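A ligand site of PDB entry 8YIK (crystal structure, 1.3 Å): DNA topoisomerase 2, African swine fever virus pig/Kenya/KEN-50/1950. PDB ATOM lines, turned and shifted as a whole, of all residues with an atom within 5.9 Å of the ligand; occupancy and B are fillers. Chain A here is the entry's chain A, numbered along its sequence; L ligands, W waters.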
ATOM      1  N   GLU A  60     -20.877  26.696 -14.591  1.00  0.00           N
ATOM      2  CA  GLU A  60     -21.724  25.647 -15.169  1.00  0.00           C
ATOM      3  C   GLU A  60     -22.139  26.004 -16.588  1.00  0.00           C
ATOM      4  O   GLU A  60     -22.135  25.139 -17.477  1.00  0.00           O
ATOM      5  CB  GLU A  60     -22.953  25.376 -14.295  1.00  0.00           C
ATOM      6  CG  GLU A  60     -22.646  24.786 -12.909  1.00  0.00           C
ATOM      7  CD  GLU A  60     -22.100  23.358 -12.912  1.00  0.00           C
ATOM      8  OE1 GLU A  60     -21.916  22.755 -13.988  1.00  0.00           O
ATOM      9  OE2 GLU A  60     -21.806  22.854 -11.813  1.00  0.00           O
ATOM     10  N   LEU A  61     -22.499  27.261 -16.836  1.00  0.00           N
ATOM     11  CA  LEU A  61     -22.888  27.696 -18.208  1.00  0.00           C
ATOM     12  C   LEU A  61     -21.667  27.632 -19.135  1.00  0.00           C
ATOM     13  O   LEU A  61     -21.818  27.173 -20.271  1.00  0.00           O
ATOM     14  CB  LEU A  61     -23.447  29.123 -18.125  1.00  0.00           C
ATOM     15  CG  LEU A  61     -24.971  29.244 -18.004  1.00  0.00           C
ATOM     16  CD1 LEU A  61     -25.569  28.147 -17.159  1.00  0.00           C
ATOM     17  CD2 LEU A  61     -25.354  30.619 -17.475  1.00  0.00           C
ATOM     18  N   ASN A  64     -20.807  24.091 -20.047  1.00  0.00           N
ATOM     19  CA  ASN A  64     -21.801  23.589 -20.994  1.00  0.00           C
ATOM     20  C   ASN A  64     -21.476  24.036 -22.422  1.00  0.00           C
ATOM     21  O   ASN A  64     -21.638  23.263 -23.375  1.00  0.00           O
ATOM     22  CB  ASN A  64     -23.206  24.035 -20.605  1.00  0.00           C
ATOM     23  CG  ASN A  64     -23.773  23.195 -19.492  1.00  0.00           C
ATOM     24  OD1 ASN A  64     -23.231  22.135 -19.169  1.00  0.00           O
ATOM     25  ND2 ASN A  64     -24.862  23.648 -18.884  1.00  0.00           N
ATOM     26  N   ALA A  65     -21.008  25.282 -22.573  1.00  0.00           N
ATOM     27  CA  ALA A  65     -20.648  25.772 -23.896  1.00  0.00           C
ATOM     28  C   ALA A  65     -19.410  25.080 -24.446  1.00  0.00           C
ATOM     29  O   ALA A  65     -19.382  24.676 -25.607  1.00  0.00           O
ATOM     30  CB  ALA A  65     -20.454  27.291 -23.842  1.00  0.00           C
ATOM     31  N   ASP A  67     -18.357  22.141 -23.615  1.00  0.00           N
ATOM     32  CA  ASP A  67     -18.755  20.755 -23.873  1.00  0.00           C
ATOM     33  C   ASP A  67     -19.375  20.616 -25.255  1.00  0.00           C
ATOM     34  O   ASP A  67     -19.184  19.605 -25.937  1.00  0.00           O
ATOM     35  CB  ASP A  67     -19.806  20.330 -22.861  1.00  0.00           C
ATOM     36  CG  ASP A  67     -19.233  19.895 -21.530  1.00  0.00           C
ATOM     37  OD1 ASP A  67     -17.982  19.823 -21.392  1.00  0.00           O
ATOM     38  OD2 ASP A  67     -20.044  19.638 -20.623  1.00  0.00           O
ATOM     39  N   HIS A  68     -20.142  21.606 -25.688  1.00  0.00           N
ATOM     40  CA  HIS A  68     -20.855  21.495 -26.982  1.00  0.00           C
ATOM     41  C   HIS A  68     -19.812  21.609 -28.084  1.00  0.00           C
ATOM     42  O   HIS A  68     -19.954  20.898 -29.054  1.00  0.00           O
ATOM     43  CB  HIS A  68     -21.876  22.625 -27.083  1.00  0.00           C
ATOM     44  CG  HIS A  68     -23.002  22.324 -28.017  1.00  0.00           C
ATOM     45  ND1 HIS A  68     -23.766  21.185 -27.917  1.00  0.00           N
ATOM     46  CD2 HIS A  68     -23.491  23.001 -29.056  1.00  0.00           C
ATOM     47  CE1 HIS A  68     -24.689  21.192 -28.867  1.00  0.00           C
ATOM     48  NE2 HIS A  68     -24.530  22.283 -29.567  1.00  0.00           N
ATOM     49  N   ASN A  95     -23.614  30.097 -27.418  1.00  0.00           N
ATOM     50  CA  ASN A  95     -22.772  29.394 -28.374  1.00  0.00           C
ATOM     51  C   ASN A  95     -23.602  29.003 -29.583  1.00  0.00           C
ATOM     52  O   ASN A  95     -24.828  28.841 -29.489  1.00  0.00           O
ATOM     53  CB  ASN A  95     -22.105  28.154 -27.749  1.00  0.00           C
ATOM     54  CG  ASN A  95     -23.104  27.201 -27.126  1.00  0.00           C
ATOM     55  OD1 ASN A  95     -23.436  27.338 -25.954  1.00  0.00           O
ATOM     56  ND2 ASN A  95     -23.572  26.220 -27.889  1.00  0.00           N
ATOM     57  N   PRO A  98     -25.460  23.150 -33.192  1.00  0.00           N
ATOM     58  CA  PRO A  98     -26.865  22.729 -33.102  1.00  0.00           C
ATOM     59  C   PRO A  98     -27.487  23.155 -31.774  1.00  0.00           C
ATOM     60  O   PRO A  98     -26.871  23.043 -30.715  1.00  0.00           O
ATOM     61  CB  PRO A  98     -26.789  21.209 -33.216  1.00  0.00           C
ATOM     62  CG  PRO A  98     -25.516  20.959 -33.954  1.00  0.00           C
ATOM     63  CD  PRO A  98     -24.558  22.035 -33.512  1.00  0.00           C
ATOM     64  N   GLY A  99     -28.713  23.656 -31.846  1.00  0.00           N
ATOM     65  CA  GLY A  99     -29.416  24.023 -30.639  1.00  0.00           C
ATOM     66  C   GLY A  99     -29.931  22.813 -29.884  1.00  0.00           C
ATOM     67  O   GLY A  99     -29.852  21.679 -30.354  1.00  0.00           O
ATOM     68  N   ILE A 100     -30.432  23.080 -28.693  1.00  0.00           N
ATOM     69  CA  ILE A 100     -31.127  22.028 -27.948  1.00  0.00           C
ATOM     70  C   ILE A 100     -32.389  21.656 -28.716  1.00  0.00           C
ATOM     71  O   ILE A 100     -33.165  22.551 -29.088  1.00  0.00           O
ATOM     72  CB  ILE A 100     -31.465  22.509 -26.531  1.00  0.00           C
ATOM     73  CG1 ILE A 100     -30.178  22.880 -25.790  1.00  0.00           C
ATOM     74  CG2 ILE A 100     -32.245  21.453 -25.774  1.00  0.00           C
ATOM     75  CD1 ILE A 100     -30.419  23.407 -24.394  1.00  0.00           C
ATOM     76  N   ALA A 122     -33.977  20.048 -19.992  1.00  0.00           N
ATOM     77  CA  ALA A 122     -32.553  20.299 -19.840  1.00  0.00           C
ATOM     78  C   ALA A 122     -32.266  21.359 -18.785  1.00  0.00           C
ATOM     79  O   ALA A 122     -31.230  21.286 -18.108  1.00  0.00           O
ATOM     80  CB  ALA A 122     -31.951  20.736 -21.168  1.00  0.00           C
ATOM     81  N   SER A 123     -33.151  22.341 -18.633  1.00  0.00           N
ATOM     82  CA  SER A 123     -32.905  23.480 -17.752  1.00  0.00           C
ATOM     83  C   SER A 123     -33.620  23.395 -16.416  1.00  0.00           C
ATOM     84  O   SER A 123     -33.209  24.088 -15.475  1.00  0.00           O
ATOM     85  CB  SER A 123     -33.305  24.789 -18.454  1.00  0.00           C
ATOM     86  OG  SER A 123     -34.673  24.777 -18.828  1.00  0.00           O
ATOM     87  N   ALA A 128     -30.939  15.302 -15.282  1.00  0.00           N
ATOM     88  CA  ALA A 128     -31.423  15.153 -16.653  1.00  0.00           C
ATOM     89  C   ALA A 128     -30.453  15.811 -17.629  1.00  0.00           C
ATOM     90  O   ALA A 128     -30.019  16.939 -17.418  1.00  0.00           O
ATOM     91  CB  ALA A 128     -32.811  15.766 -16.835  1.00  0.00           C
ATOM     92  N   GLY A 129     -30.148  15.092 -18.711  1.00  0.00           N
ATOM     93  CA  GLY A 129     -29.236  15.612 -19.710  1.00  0.00           C
ATOM     94  C   GLY A 129     -28.821  14.495 -20.657  1.00  0.00           C
ATOM     95  O   GLY A 129     -29.377  13.397 -20.614  1.00  0.00           O
ATOM     96  N   THR A 130     -27.854  14.804 -21.511  1.00  0.00           N
ATOM     97  CA  THR A 130     -27.387  13.869 -22.520  1.00  0.00           C
ATOM     98  C   THR A 130     -26.159  13.085 -22.077  1.00  0.00           C
ATOM     99  O   THR A 130     -25.616  12.297 -22.874  1.00  0.00           O
ATOM    100  CB  THR A 130     -27.108  14.580 -23.848  1.00  0.00           C
ATOM    101  OG1 THR A 130     -26.159  15.637 -23.634  1.00  0.00           O
ATOM    102  CG2 THR A 130     -28.387  15.153 -24.437  1.00  0.00           C
ATOM    103  N   ASN A 131     -25.710  13.250 -20.831  1.00  0.00           N
ATOM    104  CA  ASN A 131     -24.510  12.597 -20.340  1.00  0.00           C
ATOM    105  C   ASN A 131     -24.784  11.631 -19.188  1.00  0.00           C
ATOM    106  O   ASN A 131     -23.838  11.167 -18.557  1.00  0.00           O
ATOM    107  CB  ASN A 131     -23.466  13.635 -19.922  1.00  0.00           C
ATOM    108  CG  ASN A 131     -23.030  14.489 -21.082  1.00  0.00           C
ATOM    109  OD1 ASN A 131     -22.554  13.973 -22.096  1.00  0.00           O
ATOM    110  ND2 ASN A 131     -23.224  15.796 -20.966  1.00  0.00           N
ATOM    111  N   ILE A 132     -26.054  11.308 -18.923  1.00  0.00           N
ATOM    112  CA  ILE A 132     -26.378  10.384 -17.845  1.00  0.00           C
ATOM    113  C   ILE A 132     -25.718   9.028 -18.067  1.00  0.00           C
ATOM    114  O   ILE A 132     -25.193   8.410 -17.132  1.00  0.00           O
ATOM    115  CB  ILE A 132     -27.909  10.281 -17.685  1.00  0.00           C
ATOM    116  CG1 ILE A 132     -28.505  11.654 -17.370  1.00  0.00           C
ATOM    117  CG2 ILE A 132     -28.272   9.257 -16.610  1.00  0.00           C
ATOM    118  CD1 ILE A 132     -27.974  12.302 -16.096  1.00  0.00           C
ATOM    119  N   LYS A 140     -16.240  15.351 -22.390  1.00  0.00           N
ATOM    120  CA  LYS A 140     -17.044  16.454 -21.892  1.00  0.00           C
ATOM    121  C   LYS A 140     -16.849  16.580 -20.381  1.00  0.00           C
ATOM    122  O   LYS A 140     -16.637  15.588 -19.674  1.00  0.00           O
ATOM    123  CB  LYS A 140     -18.519  16.210 -22.181  1.00  0.00           C
ATOM    124  CG  LYS A 140     -18.903  16.331 -23.648  1.00  0.00           C
ATOM    125  CD  LYS A 140     -20.421  16.371 -23.823  1.00  0.00           C
ATOM    126  CE  LYS A 140     -20.801  16.750 -25.232  1.00  0.00           C
ATOM    127  NZ  LYS A 140     -22.285  16.811 -25.397  1.00  0.00           N
ATOM    128  N   GLY A 141     -16.881  17.821 -19.898  1.00  0.00           N
ATOM    129  CA  GLY A 141     -16.931  18.017 -18.451  1.00  0.00           C
ATOM    130  C   GLY A 141     -18.258  17.574 -17.864  1.00  0.00           C
ATOM    131  O   GLY A 141     -18.299  16.997 -16.777  1.00  0.00           O
ATOM    132  N   GLY A 142     -19.355  17.842 -18.573  1.00  0.00           N
ATOM    133  CA  GLY A 142     -20.677  17.560 -18.051  1.00  0.00           C
ATOM    134  C   GLY A 142     -20.908  16.066 -17.858  1.00  0.00           C
ATOM    135  O   GLY A 142     -20.526  15.248 -18.709  1.00  0.00           O
ATOM    136  N   THR A 143     -21.456  15.705 -16.709  1.00  0.00           N
ATOM    137  CA  THR A 143     -21.804  14.314 -16.454  1.00  0.00           C
ATOM    138  C   THR A 143     -23.109  14.095 -15.690  1.00  0.00           C
ATOM    139  O   THR A 143     -23.784  13.091 -15.935  1.00  0.00           O
ATOM    140  CB  THR A 143     -20.642  13.615 -15.735  1.00  0.00           C
ATOM    141  OG1 THR A 143     -20.977  12.247 -15.465  1.00  0.00           O
ATOM    142  CG2 THR A 143     -20.306  14.324 -14.435  1.00  0.00           C
ATOM    143  N   ASN A 144     -23.541  15.023 -14.820  1.00  0.00           N
ATOM    144  CA  ASN A 144     -24.580  14.717 -13.847  1.00  0.00           C
ATOM    145  C   ASN A 144     -25.979  15.136 -14.257  1.00  0.00           C
ATOM    146  O   ASN A 144     -26.948  14.647 -13.646  1.00  0.00           O
ATOM    147  CB  ASN A 144     -24.233  15.340 -12.496  1.00  0.00           C
ATOM    148  CG  ASN A 144     -22.918  14.847 -11.977  1.00  0.00           C
ATOM    149  OD1 ASN A 144     -22.679  13.644 -11.947  1.00  0.00           O
ATOM    150  ND2 ASN A 144     -22.041  15.773 -11.593  1.00  0.00           N
ATOM    151  N   GLY A 145     -26.137  16.003 -15.245  1.00  0.00           N
ATOM    152  CA  GLY A 145     -27.448  16.546 -15.543  1.00  0.00           C
ATOM    153  C   GLY A 145     -27.966  17.459 -14.443  1.00  0.00           C
ATOM    154  O   GLY A 145     -29.172  17.473 -14.157  1.00  0.00           O
ATOM    155  N   VAL A 146     -27.059  18.220 -13.829  1.00  0.00           N
ATOM    156  CA  VAL A 146     -27.351  19.062 -12.682  1.00  0.00           C
ATOM    157  C   VAL A 146     -27.023  20.536 -12.930  1.00  0.00           C
ATOM    158  O   VAL A 146     -27.767  21.422 -12.496  1.00  0.00           O
ATOM    159  CB  VAL A 146     -26.631  18.533 -11.421  1.00  0.00           C
ATOM    160  CG1 VAL A 146     -26.692  19.544 -10.275  1.00  0.00           C
ATOM    161  CG2 VAL A 146     -27.264  17.209 -10.991  1.00  0.00           C
ATOM    162  N   GLY A 147     -25.899  20.804 -13.610  1.00  0.00           N
ATOM    163  CA  GLY A 147     -25.317  22.140 -13.576  1.00  0.00           C
ATOM    164  C   GLY A 147     -26.232  23.255 -14.039  1.00  0.00           C
ATOM    165  O   GLY A 147     -26.280  24.329 -13.421  1.00  0.00           O
ATOM    166  N   LEU A 148     -26.968  23.049 -15.134  1.00  0.00           N
ATOM    167  CA  LEU A 148     -27.833  24.113 -15.637  1.00  0.00           C
ATOM    168  C   LEU A 148     -28.973  24.386 -14.672  1.00  0.00           C
ATOM    169  O   LEU A 148     -29.424  25.537 -14.546  1.00  0.00           O
ATOM    170  CB  LEU A 148     -28.349  23.757 -17.033  1.00  0.00           C
ATOM    171  CG  LEU A 148     -29.263  24.768 -17.733  1.00  0.00           C
ATOM    172  CD1 LEU A 148     -28.647  26.167 -17.796  1.00  0.00           C
ATOM    173  CD2 LEU A 148     -29.557  24.271 -19.139  1.00  0.00           C
ATOM    174  N   LYS A 149     -29.466  23.359 -13.989  1.00  0.00           N
ATOM    175  CA  LYS A 149     -30.511  23.558 -12.991  1.00  0.00           C
ATOM    176  C   LYS A 149     -30.003  24.386 -11.823  1.00  0.00           C
ATOM    177  O   LYS A 149     -30.760  25.179 -11.247  1.00  0.00           O
ATOM    178  CB  LYS A 149     -31.072  22.215 -12.529  1.00  0.00           C
ATOM    179  CG  LYS A 149     -32.145  21.620 -13.437  1.00  0.00           C
ATOM    180  CD  LYS A 149     -31.634  21.234 -14.832  1.00  0.00           C
ATOM    181  CE  LYS A 149     -30.514  20.213 -14.786  1.00  0.00           C
ATOM    182  NZ  LYS A 149     -30.261  19.592 -16.126  1.00  0.00           N
ATOM    183  N   THR A 193     -27.604  28.398 -28.823  1.00  0.00           N
ATOM    184  CA  THR A 193     -28.167  28.241 -27.485  1.00  0.00           C
ATOM    185  C   THR A 193     -27.649  29.383 -26.619  1.00  0.00           C
ATOM    186  O   THR A 193     -26.443  29.636 -26.592  1.00  0.00           O
ATOM    187  CB  THR A 193     -27.787  26.893 -26.861  1.00  0.00           C
ATOM    188  OG1 THR A 193     -28.234  25.845 -27.723  1.00  0.00           O
ATOM    189  CG2 THR A 193     -28.416  26.725 -25.489  1.00  0.00           C
ATOM    190  N   ILE A 195     -28.166  31.288 -22.679  1.00  0.00           N
ATOM    191  CA  ILE A 195     -28.712  31.403 -21.321  1.00  0.00           C
ATOM    192  C   ILE A 195     -28.365  32.787 -20.817  1.00  0.00           C
ATOM    193  O   ILE A 195     -27.198  33.190 -20.826  1.00  0.00           O
ATOM    194  CB  ILE A 195     -28.130  30.344 -20.373  1.00  0.00           C
ATOM    195  CG1 ILE A 195     -28.258  28.927 -20.960  1.00  0.00           C
ATOM    196  CG2 ILE A 195     -28.811  30.448 -19.002  1.00  0.00           C
ATOM    197  CD1 ILE A 195     -29.685  28.444 -21.149  1.00  0.00           C
ATOM    198  N   GLN A 366     -20.106  17.556  -7.665  1.00  0.00           N
ATOM    199  CA  GLN A 366     -20.650  18.365  -8.746  1.00  0.00           C
ATOM    200  C   GLN A 366     -19.747  19.538  -9.095  1.00  0.00           C
ATOM    201  O   GLN A 366     -19.647  19.919 -10.269  1.00  0.00           O
ATOM    202  CB  GLN A 366     -22.050  18.869  -8.400  1.00  0.00           C
ATOM    203  CG  GLN A 366     -22.650  19.869  -9.404  1.00  0.00           C
ATOM    204  CD  GLN A 366     -22.979  19.238 -10.733  1.00  0.00           C
ATOM    205  OE1 GLN A 366     -23.365  18.071 -10.802  1.00  0.00           O
ATOM    206  NE2 GLN A 366     -22.840  20.011 -11.806  1.00  0.00           N
ATOM    207  N   LYS A 368     -16.586  19.633  -9.289  1.00  0.00           N
ATOM    208  CA  LYS A 368     -15.466  19.206 -10.115  1.00  0.00           C
ATOM    209  C   LYS A 368     -14.182  19.948  -9.735  1.00  0.00           C
ATOM    210  O   LYS A 368     -13.439  20.457 -10.577  1.00  0.00           O
ATOM    211  CB  LYS A 368     -15.797  19.304 -11.614  1.00  0.00           C
ATOM    212  CG  LYS A 368     -17.107  18.596 -11.950  1.00  0.00           C
ATOM    213  CD  LYS A 368     -17.486  18.741 -13.418  1.00  0.00           C
ATOM    214  CE  LYS A 368     -18.826  18.090 -13.712  1.00  0.00           C
ATOM    215  NZ  LYS A 368     -19.958  18.819 -13.104  1.00  0.00           N
HETATM  216  P1  LIG L   1     -23.354  18.476 -15.311  1.00  0.00           P
HETATM  217  O1  LIG L   1     -22.984  19.862 -15.816  1.00  0.00           O
HETATM  218  O2  LIG L   1     -24.432  18.511 -14.266  1.00  0.00           O
HETATM  219  O3  LIG L   1     -22.136  17.690 -14.869  1.00  0.00           O
HETATM  220  P2  LIG L   1     -24.618  18.212 -18.006  1.00  0.00           P
HETATM  221  O4  LIG L   1     -23.807  19.324 -18.595  1.00  0.00           O
HETATM  222  O5  LIG L   1     -24.965  17.040 -18.863  1.00  0.00           O
HETATM  223  O6  LIG L   1     -23.941  17.697 -16.634  1.00  0.00           O
HETATM  224  P3  LIG L   1     -26.539  20.344 -17.464  1.00  0.00           P
HETATM  225  O7  LIG L   1     -25.398  21.274 -17.288  1.00  0.00           O
HETATM  226  O8  LIG L   1     -27.665  20.414 -16.489  1.00  0.00           O
HETATM  227  O9  LIG L   1     -25.988  18.835 -17.445  1.00  0.00           O
HETATM  228  O10 LIG L   1     -27.108  20.483 -18.961  1.00  0.00           O
HETATM  229  C1  LIG L   1     -28.227  19.648 -19.336  1.00  0.00           C
HETATM  230  C2  LIG L   1     -28.120  19.306 -20.803  1.00  0.00           C
HETATM  231  O11 LIG L   1     -28.480  20.470 -21.603  1.00  0.00           O
HETATM  232  C3  LIG L   1     -26.731  18.921 -21.302  1.00  0.00           C
HETATM  233  O12 LIG L   1     -26.457  17.545 -21.060  1.00  0.00           O
HETATM  234  C4  LIG L   1     -26.825  19.250 -22.799  1.00  0.00           C
HETATM  235  O13 LIG L   1     -27.456  18.211 -23.507  1.00  0.00           O
HETATM  236  C5  LIG L   1     -27.713  20.494 -22.795  1.00  0.00           C
HETATM  237  N1  LIG L   1     -27.031  21.771 -22.841  1.00  0.00           N
HETATM  238  C6  LIG L   1     -26.730  22.575 -21.769  1.00  0.00           C
HETATM  239  N2  LIG L   1     -26.124  23.683 -22.122  1.00  0.00           N
HETATM  240  C7  LIG L   1     -26.008  23.602 -23.507  1.00  0.00           C
HETATM  241  C8  LIG L   1     -25.443  24.468 -24.458  1.00  0.00           C
HETATM  242  N3  LIG L   1     -24.866  25.626 -24.151  1.00  0.00           N
HETATM  243  N4  LIG L   1     -25.501  24.082 -25.749  1.00  0.00           N
HETATM  244  C9  LIG L   1     -26.087  22.913 -26.054  1.00  0.00           C
HETATM  245  N5  LIG L   1     -26.643  22.016 -25.236  1.00  0.00           N
HETATM  246  C10 LIG L   1     -26.569  22.433 -23.957  1.00  0.00           C
HETATM  247  O   HOH W   1     -22.724  19.443 -21.117  1.00  0.00           O
HETATM  248  O   HOH W   2     -22.887  22.712 -16.376  1.00  0.00           O
HETATM  249  O   HOH W   3     -26.341  14.776 -18.415  1.00  0.00           O
HETATM  250  O   HOH W   4     -23.536  21.172 -23.213  1.00  0.00           O
HETATM  251  O   HOH W   5     -24.097  29.024 -24.013  1.00  0.00           O
HETATM  252  O   HOH W   6     -24.171  27.377 -21.704  1.00  0.00           O
HETATM  253  O   HOH W   7     -19.958  21.302 -15.308  1.00  0.00           O
HETATM  254  O   HOH W   8     -27.648  19.806 -26.575  1.00  0.00           O
HETATM  255  O   HOH W   9     -25.686  17.852 -26.057  1.00  0.00           O
HETATM  256  O   HOH W  10     -21.163  20.702 -17.894  1.00  0.00           O
HETATM  257  O   HOH W  11     -26.059  25.887 -20.313  1.00  0.00           O
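N of Val 146 sits at hydrogen-bond distance from O2 of the ligand (2.7 Å). The side-chain amino group of Lys 149 is in salt-bridge range of an oxygen (O8) of the ligand (2.7 Å). O3 of the ligand sits at hydrogen-bond distance from N of Thr 143 (2.8 Å). N of Gly 147 sits at hydrogen-bond distance from O2 of the ligand (2.8 Å). The side-chain amide oxygen (OD1) of Asn 95 is in hydrogen-bond range of a nitrogen (N3) of the ligand (2.9 Å). The backbone NH of Thr 130 is in hydrogen-bond range of an oxygen (O12) of the ligand, 3.1 Å away. An oxygen (O13) of the ligand lies within hydrogen-bond range of the side-chain hydroxyl (OG1) of Thr 130. ND2 of Asn 64 sits at hydrogen-bond distance from O7 of the ligand. The side-chain amide nitrogen (ND2) of Asn 131 is in hydrogen-bond range of an oxygen (O5) of the ligand (3.0 Å). N of Asn 144 is in hydrogen-bond range of O3 of the ligand (3.0 Å). O3 of the ligand is in salt-bridge range of NZ of Lys 368. The backbone NH (N) of Leu 148 lies within hydrogen-bond range of an oxygen (O8) of the ligand, at 3.0 Å. The backbone NH (N) of Gly 145 sits at hydrogen-bond distance from an oxygen (O6) of the ligand (3.1 Å). The side-chain amide nitrogen (NE2) of Gln 366 lies within hydrogen-bond range of an oxygen (O2) of the ligand.
The side-chain amino group of Lys 149 sits at hydrogen-bond distance from the backbone carbonyl oxygen of Gly 145. The backbone carbonyl oxygen (O) of Ala 122 is in hydrogen-bond range of the side-chain amino group (NZ) of Lys 149, 2.8 Å away. The side-chain amino group (NZ) of Lys 149 is in hydrogen-bond range of the backbone carbonyl oxygen (O) of Ala 128, 3.0 Å away. The side-chain amide nitrogen (ND2) of Asn 64 lies close to the backbone carbonyl oxygen (O) of Glu 60 (3.4 Å). ND2 of Asn 144 is in hydrogen-bond range of OE1 of Gln 366 (2.8 Å). O of Gln 366 lies within hydrogen-bond range of NZ of Lys 368 (3.1 Å). The backbone carbonyl oxygen (O) of Gly 145 is in hydrogen-bond range of the backbone NH (N) of Ala 128. A ring nitrogen (NE2) of His 68 lies within hydrogen-bond range of the backbone carbonyl oxygen (O) of Pro 98, 2.7 Å away.
Residues that only touch the ligand: His 68, Gly 142, Ala 122, Glu 60, Gly 129, Ile 100, Ala 128 and Thr 193. Hydrophobic or aromatic side chains within 4 Å of the ligand: His 68, Ile 100, Ala 122, Val 146 and Leu 148. 21 residues have an atom within 4 Å of the ligand: Glu 60, Asn 64, His 68, Asn 95, Ile 100, Ala 122, Ala 128, Gly 129, Thr 130, Asn 131, Gly 142, Thr 143, Asn 144, Gly 145, Val 146, Gly 147, Leu 148, Lys 149, Thr 193, Gln 366 and Lys 368.
Water W1 lies within hydrogen-bond range of the side-chain carboxylate of Asp 67 (2.7 Å), an oxygen (O4) of the ligand (2.7 Å) and the side-chain amide oxygen of Asn 64 (3.4 Å). Water W11 lies within hydrogen-bond range of N2 of the ligand (2.9 Å) and ND2 of Asn 64 (2.9 Å). Water W10 lies within hydrogen-bond range of OD1 of Asn 64, O1 of the ligand, OD2 of Asp 67 and N of Gly 142. Water W2 lies within hydrogen-bond range of OE1 of Glu 60 (2.6 Å), OD1 of Asn 64 (2.9 Å) and O1 of the ligand (2.9 Å). Water W6 lies within hydrogen-bond range of the backbone carbonyl oxygen of Leu 61 and a nitrogen (N3) of the ligand. Water W5 bridges the side-chain amide oxygen of Asn 95 (2.7 Å) and a nitrogen (N3) of the ligand (3.5 Å).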
